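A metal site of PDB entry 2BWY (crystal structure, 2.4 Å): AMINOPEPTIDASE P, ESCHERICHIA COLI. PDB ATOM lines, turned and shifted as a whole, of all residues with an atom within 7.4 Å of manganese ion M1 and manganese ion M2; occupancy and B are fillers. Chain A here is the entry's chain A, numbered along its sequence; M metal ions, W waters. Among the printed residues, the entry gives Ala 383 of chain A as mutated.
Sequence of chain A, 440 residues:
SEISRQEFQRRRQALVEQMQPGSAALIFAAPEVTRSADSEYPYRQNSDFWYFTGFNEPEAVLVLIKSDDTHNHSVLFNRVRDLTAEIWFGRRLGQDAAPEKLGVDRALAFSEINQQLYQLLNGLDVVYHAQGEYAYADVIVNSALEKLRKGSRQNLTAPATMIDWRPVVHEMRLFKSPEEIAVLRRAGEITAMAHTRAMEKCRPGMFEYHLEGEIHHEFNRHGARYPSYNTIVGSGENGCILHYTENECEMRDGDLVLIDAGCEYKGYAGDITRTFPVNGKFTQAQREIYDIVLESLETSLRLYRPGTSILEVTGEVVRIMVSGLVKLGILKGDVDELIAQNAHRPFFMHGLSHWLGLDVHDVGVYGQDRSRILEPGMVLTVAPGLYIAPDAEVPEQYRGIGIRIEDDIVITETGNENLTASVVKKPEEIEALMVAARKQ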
ATOM      1  N   TYR A 229     -14.952 -15.482 -33.778  1.00  0.00           N
ATOM      2  CA  TYR A 229     -14.203 -16.534 -33.083  1.00  0.00           C
ATOM      3  C   TYR A 229     -15.143 -17.712 -32.815  1.00  0.00           C
ATOM      4  O   TYR A 229     -16.364 -17.592 -32.969  1.00  0.00           O
ATOM      5  CB  TYR A 229     -13.593 -16.013 -31.767  1.00  0.00           C
ATOM      6  CG  TYR A 229     -14.588 -15.371 -30.864  1.00  0.00           C
ATOM      7  CD1 TYR A 229     -14.933 -14.039 -31.021  1.00  0.00           C
ATOM      8  CD2 TYR A 229     -15.215 -16.090 -29.854  1.00  0.00           C
ATOM      9  CE1 TYR A 229     -15.864 -13.446 -30.210  1.00  0.00           C
ATOM     10  CE2 TYR A 229     -16.152 -15.506 -29.033  1.00  0.00           C
ATOM     11  CZ  TYR A 229     -16.458 -14.174 -29.217  1.00  0.00           C
ATOM     12  OH  TYR A 229     -17.384 -13.556 -28.433  1.00  0.00           O
ATOM     13  N   ILE A 232     -18.516 -20.112 -27.740  1.00  0.00           N
ATOM     14  CA  ILE A 232     -18.462 -20.787 -26.458  1.00  0.00           C
ATOM     15  C   ILE A 232     -19.855 -20.866 -25.850  1.00  0.00           C
ATOM     16  O   ILE A 232     -20.529 -19.859 -25.689  1.00  0.00           O
ATOM     17  CB  ILE A 232     -17.514 -20.016 -25.487  1.00  0.00           C
ATOM     18  CG1 ILE A 232     -16.068 -20.035 -26.029  1.00  0.00           C
ATOM     19  CG2 ILE A 232     -17.575 -20.579 -24.061  1.00  0.00           C
ATOM     20  CD1 ILE A 232     -15.261 -18.833 -25.642  1.00  0.00           C
ATOM     21  N   HIS A 243     -12.244 -21.091 -22.728  1.00  0.00           N
ATOM     22  CA  HIS A 243     -12.542 -21.218 -24.171  1.00  0.00           C
ATOM     23  C   HIS A 243     -13.071 -22.640 -24.460  1.00  0.00           C
ATOM     24  O   HIS A 243     -12.491 -23.403 -25.238  1.00  0.00           O
ATOM     25  CB  HIS A 243     -11.327 -20.802 -25.035  1.00  0.00           C
ATOM     26  CG  HIS A 243     -10.867 -19.373 -24.816  1.00  0.00           C
ATOM     27  ND1 HIS A 243      -9.541 -18.984 -24.960  1.00  0.00           N
ATOM     28  CD2 HIS A 243     -11.539 -18.255 -24.468  1.00  0.00           C
ATOM     29  CE1 HIS A 243      -9.435 -17.688 -24.711  1.00  0.00           C
ATOM     30  NE2 HIS A 243     -10.634 -17.224 -24.409  1.00  0.00           N
ATOM     31  N   ILE A 259     -22.507 -18.041 -22.356  1.00  0.00           N
ATOM     32  CA  ILE A 259     -22.380 -17.932 -23.809  1.00  0.00           C
ATOM     33  C   ILE A 259     -21.419 -16.827 -24.167  1.00  0.00           C
ATOM     34  O   ILE A 259     -21.659 -15.674 -23.840  1.00  0.00           O
ATOM     35  CB  ILE A 259     -23.715 -17.653 -24.492  1.00  0.00           C
ATOM     36  CG1 ILE A 259     -24.731 -18.720 -24.097  1.00  0.00           C
ATOM     37  CG2 ILE A 259     -23.527 -17.635 -26.003  1.00  0.00           C
ATOM     38  CD1 ILE A 259     -25.975 -18.685 -24.945  1.00  0.00           C
ATOM     39  N   ASP A 260     -20.327 -17.189 -24.845  1.00  0.00           N
ATOM     40  CA  ASP A 260     -19.379 -16.213 -25.370  1.00  0.00           C
ATOM     41  C   ASP A 260     -19.351 -16.316 -26.901  1.00  0.00           C
ATOM     42  O   ASP A 260     -18.856 -17.292 -27.471  1.00  0.00           O
ATOM     43  CB  ASP A 260     -17.977 -16.447 -24.782  1.00  0.00           C
ATOM     44  CG  ASP A 260     -17.060 -15.223 -24.924  1.00  0.00           C
ATOM     45  OD1 ASP A 260     -17.280 -14.339 -25.798  1.00  0.00           O
ATOM     46  OD2 ASP A 260     -16.098 -15.161 -24.136  1.00  0.00           O
ATOM     47  N   ALA A 261     -19.893 -15.284 -27.550  1.00  0.00           N
ATOM     48  CA  ALA A 261     -20.058 -15.305 -28.993  1.00  0.00           C
ATOM     49  C   ALA A 261     -20.071 -13.909 -29.593  1.00  0.00           C
ATOM     50  O   ALA A 261     -20.537 -12.921 -28.984  1.00  0.00           O
ATOM     51  CB  ALA A 261     -21.320 -16.032 -29.359  1.00  0.00           C
ATOM     52  N   GLY A 262     -19.582 -13.835 -30.821  1.00  0.00           N
ATOM     53  CA  GLY A 262     -19.363 -12.570 -31.504  1.00  0.00           C
ATOM     54  C   GLY A 262     -19.425 -12.785 -32.991  1.00  0.00           C
ATOM     55  O   GLY A 262     -18.964 -13.814 -33.483  1.00  0.00           O
ATOM     56  N   GLY A 270     -17.679  -8.364 -33.150  1.00  0.00           N
ATOM     57  CA  GLY A 270     -18.452  -8.241 -31.930  1.00  0.00           C
ATOM     58  C   GLY A 270     -17.893  -9.246 -30.948  1.00  0.00           C
ATOM     59  O   GLY A 270     -17.285 -10.252 -31.356  1.00  0.00           O
ATOM     60  N   ASP A 271     -18.079  -8.993 -29.662  1.00  0.00           N
ATOM     61  CA  ASP A 271     -17.619  -9.923 -28.629  1.00  0.00           C
ATOM     62  C   ASP A 271     -18.400  -9.741 -27.324  1.00  0.00           C
ATOM     63  O   ASP A 271     -18.078  -8.876 -26.514  1.00  0.00           O
ATOM     64  CB  ASP A 271     -16.122  -9.715 -28.402  1.00  0.00           C
ATOM     65  CG  ASP A 271     -15.552 -10.653 -27.399  1.00  0.00           C
ATOM     66  OD1 ASP A 271     -16.316 -11.490 -26.854  1.00  0.00           O
ATOM     67  OD2 ASP A 271     -14.335 -10.544 -27.147  1.00  0.00           O
ATOM     68  N   ILE A 272     -19.413 -10.572 -27.121  1.00  0.00           N
ATOM     69  CA  ILE A 272     -20.246 -10.471 -25.937  1.00  0.00           C
ATOM     70  C   ILE A 272     -20.226 -11.794 -25.180  1.00  0.00           C
ATOM     71  O   ILE A 272     -20.225 -12.873 -25.795  1.00  0.00           O
ATOM     72  CB  ILE A 272     -21.699 -10.154 -26.294  1.00  0.00           C
ATOM     73  CG1 ILE A 272     -21.811  -8.812 -27.013  1.00  0.00           C
ATOM     74  CG2 ILE A 272     -22.589 -10.142 -25.016  1.00  0.00           C
ATOM     75  CD1 ILE A 272     -23.239  -8.432 -27.340  1.00  0.00           C
ATOM     76  N   THR A 273     -20.217 -11.689 -23.851  1.00  0.00           N
ATOM     77  CA  THR A 273     -20.492 -12.835 -22.981  1.00  0.00           C
ATOM     78  C   THR A 273     -21.687 -12.521 -22.121  1.00  0.00           C
ATOM     79  O   THR A 273     -21.774 -11.431 -21.552  1.00  0.00           O
ATOM     80  CB  THR A 273     -19.308 -13.244 -22.063  1.00  0.00           C
ATOM     81  OG1 THR A 273     -18.083 -13.292 -22.813  1.00  0.00           O
ATOM     82  CG2 THR A 273     -19.568 -14.619 -21.467  1.00  0.00           C
ATOM     83  N   LEU A 352      -9.050  -8.282 -17.710  1.00  0.00           N
ATOM     84  CA  LEU A 352     -10.397  -7.683 -17.780  1.00  0.00           C
ATOM     85  C   LEU A 352     -10.783  -7.232 -19.188  1.00  0.00           C
ATOM     86  O   LEU A 352     -11.949  -7.279 -19.549  1.00  0.00           O
ATOM     87  CB  LEU A 352     -10.421  -6.462 -16.845  1.00  0.00           C
ATOM     88  CG  LEU A 352     -11.749  -5.725 -16.685  1.00  0.00           C
ATOM     89  CD1 LEU A 352     -12.751  -6.600 -15.997  1.00  0.00           C
ATOM     90  CD2 LEU A 352     -11.506  -4.471 -15.889  1.00  0.00           C
ATOM     91  N   SER A 353      -9.810  -6.787 -19.966  1.00  0.00           N
ATOM     92  CA  SER A 353     -10.075  -6.023 -21.187  1.00  0.00           C
ATOM     93  C   SER A 353      -9.047  -6.289 -22.279  1.00  0.00           C
ATOM     94  O   SER A 353      -7.863  -6.363 -21.987  1.00  0.00           O
ATOM     95  CB  SER A 353     -10.095  -4.521 -20.867  1.00  0.00           C
ATOM     96  OG  SER A 353     -11.236  -4.161 -20.099  1.00  0.00           O
ATOM     97  N   HIS A 354      -9.503  -6.474 -23.522  1.00  0.00           N
ATOM     98  CA  HIS A 354      -8.598  -6.490 -24.670  1.00  0.00           C
ATOM     99  C   HIS A 354      -9.104  -5.535 -25.732  1.00  0.00           C
ATOM    100  O   HIS A 354     -10.279  -5.199 -25.747  1.00  0.00           O
ATOM    101  CB  HIS A 354      -8.412  -7.912 -25.237  1.00  0.00           C
ATOM    102  CG  HIS A 354      -9.683  -8.597 -25.635  1.00  0.00           C
ATOM    103  ND1 HIS A 354     -10.305  -8.396 -26.848  1.00  0.00           N
ATOM    104  CD2 HIS A 354     -10.448  -9.512 -24.971  1.00  0.00           C
ATOM    105  CE1 HIS A 354     -11.400  -9.141 -26.913  1.00  0.00           C
ATOM    106  NE2 HIS A 354     -11.505  -9.824 -25.794  1.00  0.00           N
ATOM    107  N   TRP A 355      -8.211  -5.102 -26.624  1.00  0.00           N
ATOM    108  CA  TRP A 355      -8.588  -4.261 -27.749  1.00  0.00           C
ATOM    109  C   TRP A 355      -9.503  -5.073 -28.672  1.00  0.00           C
ATOM    110  O   TRP A 355      -9.385  -6.281 -28.764  1.00  0.00           O
ATOM    111  CB  TRP A 355      -7.370  -3.802 -28.574  1.00  0.00           C
ATOM    112  CG  TRP A 355      -6.220  -3.190 -27.842  1.00  0.00           C
ATOM    113  CD1 TRP A 355      -4.911  -3.549 -27.955  1.00  0.00           C
ATOM    114  CD2 TRP A 355      -6.258  -2.080 -26.926  1.00  0.00           C
ATOM    115  NE1 TRP A 355      -4.136  -2.755 -27.158  1.00  0.00           N
ATOM    116  CE2 TRP A 355      -4.935  -1.846 -26.512  1.00  0.00           C
ATOM    117  CE3 TRP A 355      -7.277  -1.281 -26.401  1.00  0.00           C
ATOM    118  CZ2 TRP A 355      -4.602  -0.850 -25.595  1.00  0.00           C
ATOM    119  CZ3 TRP A 355      -6.951  -0.292 -25.515  1.00  0.00           C
ATOM    120  CH2 TRP A 355      -5.617  -0.088 -25.109  1.00  0.00           C
ATOM    121  N   LEU A 356     -10.396  -4.386 -29.365  1.00  0.00           N
ATOM    122  CA  LEU A 356     -11.334  -5.009 -30.277  1.00  0.00           C
ATOM    123  C   LEU A 356     -11.342  -4.263 -31.625  1.00  0.00           C
ATOM    124  O   LEU A 356     -11.332  -3.040 -31.674  1.00  0.00           O
ATOM    125  CB  LEU A 356     -12.717  -4.987 -29.631  1.00  0.00           C
ATOM    126  CG  LEU A 356     -13.869  -5.725 -30.305  1.00  0.00           C
ATOM    127  CD1 LEU A 356     -13.737  -7.224 -30.157  1.00  0.00           C
ATOM    128  CD2 LEU A 356     -15.177  -5.206 -29.706  1.00  0.00           C
ATOM    129  N   VAL A 360     -10.711 -10.019 -32.982  1.00  0.00           N
ATOM    130  CA  VAL A 360     -11.363 -10.016 -31.661  1.00  0.00           C
ATOM    131  C   VAL A 360     -10.331  -9.672 -30.550  1.00  0.00           C
ATOM    132  O   VAL A 360     -10.612  -8.867 -29.656  1.00  0.00           O
ATOM    133  CB  VAL A 360     -12.136 -11.339 -31.387  1.00  0.00           C
ATOM    134  CG1 VAL A 360     -11.210 -12.551 -31.432  1.00  0.00           C
ATOM    135  CG2 VAL A 360     -12.854 -11.302 -30.048  1.00  0.00           C
ATOM    136  N   HIS A 361      -9.140 -10.252 -30.637  1.00  0.00           N
ATOM    137  CA  HIS A 361      -8.009  -9.857 -29.810  1.00  0.00           C
ATOM    138  C   HIS A 361      -7.153  -8.943 -30.653  1.00  0.00           C
ATOM    139  O   HIS A 361      -6.187  -9.387 -31.306  1.00  0.00           O
ATOM    140  CB  HIS A 361      -7.212 -11.065 -29.329  1.00  0.00           C
ATOM    141  CG  HIS A 361      -7.961 -11.969 -28.418  1.00  0.00           C
ATOM    142  ND1 HIS A 361      -7.583 -13.262 -28.176  1.00  0.00           N
ATOM    143  CD2 HIS A 361      -9.090 -11.770 -27.695  1.00  0.00           C
ATOM    144  CE1 HIS A 361      -8.425 -13.824 -27.328  1.00  0.00           C
ATOM    145  NE2 HIS A 361      -9.352 -12.932 -27.026  1.00  0.00           N
ATOM    146  N   THR A 381     -12.962  -4.557 -24.876  1.00  0.00           N
ATOM    147  CA  THR A 381     -13.897  -5.323 -24.074  1.00  0.00           C
ATOM    148  C   THR A 381     -13.772  -5.076 -22.570  1.00  0.00           C
ATOM    149  O   THR A 381     -12.724  -4.641 -22.073  1.00  0.00           O
ATOM    150  CB  THR A 381     -13.779  -6.821 -24.367  1.00  0.00           C
ATOM    151  OG1 THR A 381     -12.520  -7.325 -23.871  1.00  0.00           O
ATOM    152  CG2 THR A 381     -13.912  -7.059 -25.878  1.00  0.00           C
ATOM    153  N   VAL A 382     -14.880  -5.320 -21.854  1.00  0.00           N
ATOM    154  CA  VAL A 382     -14.914  -5.290 -20.399  1.00  0.00           C
ATOM    155  C   VAL A 382     -15.561  -6.612 -20.020  1.00  0.00           C
ATOM    156  O   VAL A 382     -16.747  -6.825 -20.286  1.00  0.00           O
ATOM    157  CB  VAL A 382     -15.718  -4.087 -19.859  1.00  0.00           C
ATOM    158  CG1 VAL A 382     -15.474  -3.908 -18.346  1.00  0.00           C
ATOM    159  CG2 VAL A 382     -15.326  -2.799 -20.596  1.00  0.00           C
ATOM    160  N   ALA A 383     -14.783  -7.508 -19.412  1.00  0.00           N
ATOM    161  CA  ALA A 383     -15.149  -8.910 -19.280  1.00  0.00           C
ATOM    162  C   ALA A 383     -14.701  -9.534 -17.958  1.00  0.00           C
ATOM    163  O   ALA A 383     -13.911 -10.462 -17.956  1.00  0.00           O
ATOM    164  CB  ALA A 383     -14.555  -9.707 -20.449  1.00  0.00           C
ATOM    165  N   ARG A 404     -19.237 -15.216 -16.563  1.00  0.00           N
ATOM    166  CA  ARG A 404     -18.607 -14.067 -17.179  1.00  0.00           C
ATOM    167  C   ARG A 404     -19.682 -13.216 -17.810  1.00  0.00           C
ATOM    168  O   ARG A 404     -20.692 -13.730 -18.298  1.00  0.00           O
ATOM    169  CB  ARG A 404     -17.583 -14.504 -18.242  1.00  0.00           C
ATOM    170  CG  ARG A 404     -16.925 -13.357 -19.028  1.00  0.00           C
ATOM    171  CD  ARG A 404     -15.664 -13.786 -19.777  1.00  0.00           C
ATOM    172  NE  ARG A 404     -15.862 -14.761 -20.876  1.00  0.00           N
ATOM    173  CZ  ARG A 404     -15.617 -16.079 -20.804  1.00  0.00           C
ATOM    174  NH1 ARG A 404     -15.187 -16.649 -19.695  1.00  0.00           N
ATOM    175  NH2 ARG A 404     -15.801 -16.846 -21.864  1.00  0.00           N
ATOM    176  N   GLU A 406     -19.621  -9.798 -20.406  1.00  0.00           N
ATOM    177  CA  GLU A 406     -18.702  -9.044 -21.249  1.00  0.00           C
ATOM    178  C   GLU A 406     -19.467  -8.165 -22.223  1.00  0.00           C
ATOM    179  O   GLU A 406     -20.406  -8.609 -22.874  1.00  0.00           O
ATOM    180  CB  GLU A 406     -17.774 -10.017 -21.990  1.00  0.00           C
ATOM    181  CG  GLU A 406     -16.988  -9.434 -23.124  1.00  0.00           C
ATOM    182  CD  GLU A 406     -15.982 -10.395 -23.669  1.00  0.00           C
ATOM    183  OE1 GLU A 406     -16.317 -11.595 -23.801  1.00  0.00           O
ATOM    184  OE2 GLU A 406     -14.863  -9.937 -24.004  1.00  0.00           O
ATOM    185  N   ASP A 407     -19.037  -6.907 -22.281  1.00  0.00           N
ATOM    186  CA  ASP A 407     -19.565  -5.861 -23.147  1.00  0.00           C
ATOM    187  C   ASP A 407     -18.393  -5.264 -23.947  1.00  0.00           C
ATOM    188  O   ASP A 407     -17.237  -5.398 -23.538  1.00  0.00           O
ATOM    189  CB  ASP A 407     -20.202  -4.754 -22.311  1.00  0.00           C
ATOM    190  CG  ASP A 407     -21.699  -4.976 -22.046  1.00  0.00           C
ATOM    191  OD1 ASP A 407     -22.349  -5.735 -22.804  1.00  0.00           O
ATOM    192  OD2 ASP A 407     -22.234  -4.351 -21.095  1.00  0.00           O
ATOM    193  N   ASP A 408     -18.731  -4.617 -25.066  1.00  0.00           N
ATOM    194  CA  ASP A 408     -17.757  -3.963 -25.958  1.00  0.00           C
ATOM    195  C   ASP A 408     -17.985  -2.458 -25.873  1.00  0.00           C
ATOM    196  O   ASP A 408     -19.126  -1.987 -25.939  1.00  0.00           O
ATOM    197  CB  ASP A 408     -17.931  -4.422 -27.413  1.00  0.00           C
ATOM    198  CG  ASP A 408     -17.936  -5.941 -27.578  1.00  0.00           C
ATOM    199  OD1 ASP A 408     -17.300  -6.659 -26.768  1.00  0.00           O
ATOM    200  OD2 ASP A 408     -18.577  -6.423 -28.520  1.00  0.00           O
HETATM  201 MN    MN M   1     -15.742 -12.898 -25.325  1.00  0.00          MN
HETATM  202 MN    MN M   2     -13.250 -11.131 -25.310  1.00  0.00          MN
HETATM  203  O   HOH W   1     -12.789 -13.687 -26.176  1.00  0.00           O
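OD1 of Asp 271 lies close to OH of Tyr 229 (2.8 Å). N of Asp 271 lies within hydrogen-bond range of OD2 of Asp 408 (2.9 Å). The side-chain hydroxyl (OG1) of Thr 273 lies close to the side-chain carboxylate (OD2) of Asp 260 (3.0 Å). The side-chain hydroxyl (OH) of Tyr 229 lies close to the side-chain carboxylate (OD1) of Asp 260, 2.8 Å away. The side-chain carboxylate (OD2) of Asp 260 sits close to the guanidinium group (NH2) of Arg 404, at 2.8 Å. The backbone carbonyl oxygen of His 354 sits at hydrogen-bond distance from the backbone NH of Thr 381 (2.9 Å). The side-chain hydroxyl of Thr 273 is in hydrogen-bond range of the guanidinium group of Arg 404 (3.3 Å). The side-chain hydroxyl (OH) of Tyr 229 lies close to the backbone NH (N) of Ala 261 (3.2 Å).
Manganese ion M2 is bound by OD2 of Asp 271 (2.2 Å), NE2 of His 354 (2.2 Å) and OE2 of Glu 406 (2.4 Å). Manganese ion M2 has three donor atoms within binding distance. Slightly farther from manganese ion M2 lies water W1 (2.7 Å).
Residues that only touch manganese ion M1: Thr 273 (3.5 Å) and Tyr 229 (3.6 Å). Within 4 Å of manganese ion M1: Tyr 229, Asp 260, Asp 271, Thr 273 and Glu 406. The nearest printed residue that does not touch manganese ion M1 is Ile 272 (4.5 Å).
Manganese ion M1 is bound by the side-chain carboxylate (OE1) of Glu 406, the side-chain carboxylate (OD1) of Asp 271, the side-chain carboxylate (OD1) of Asp 260 and the side-chain carboxylate (OD2) of Asp 260.
Three residues have an atom within 4 Å of manganese ion M2: Asp 271, His 354 and Glu 406. The nearest printed residue that does not touch manganese ion M2 is Thr 381 (4.1 Å).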
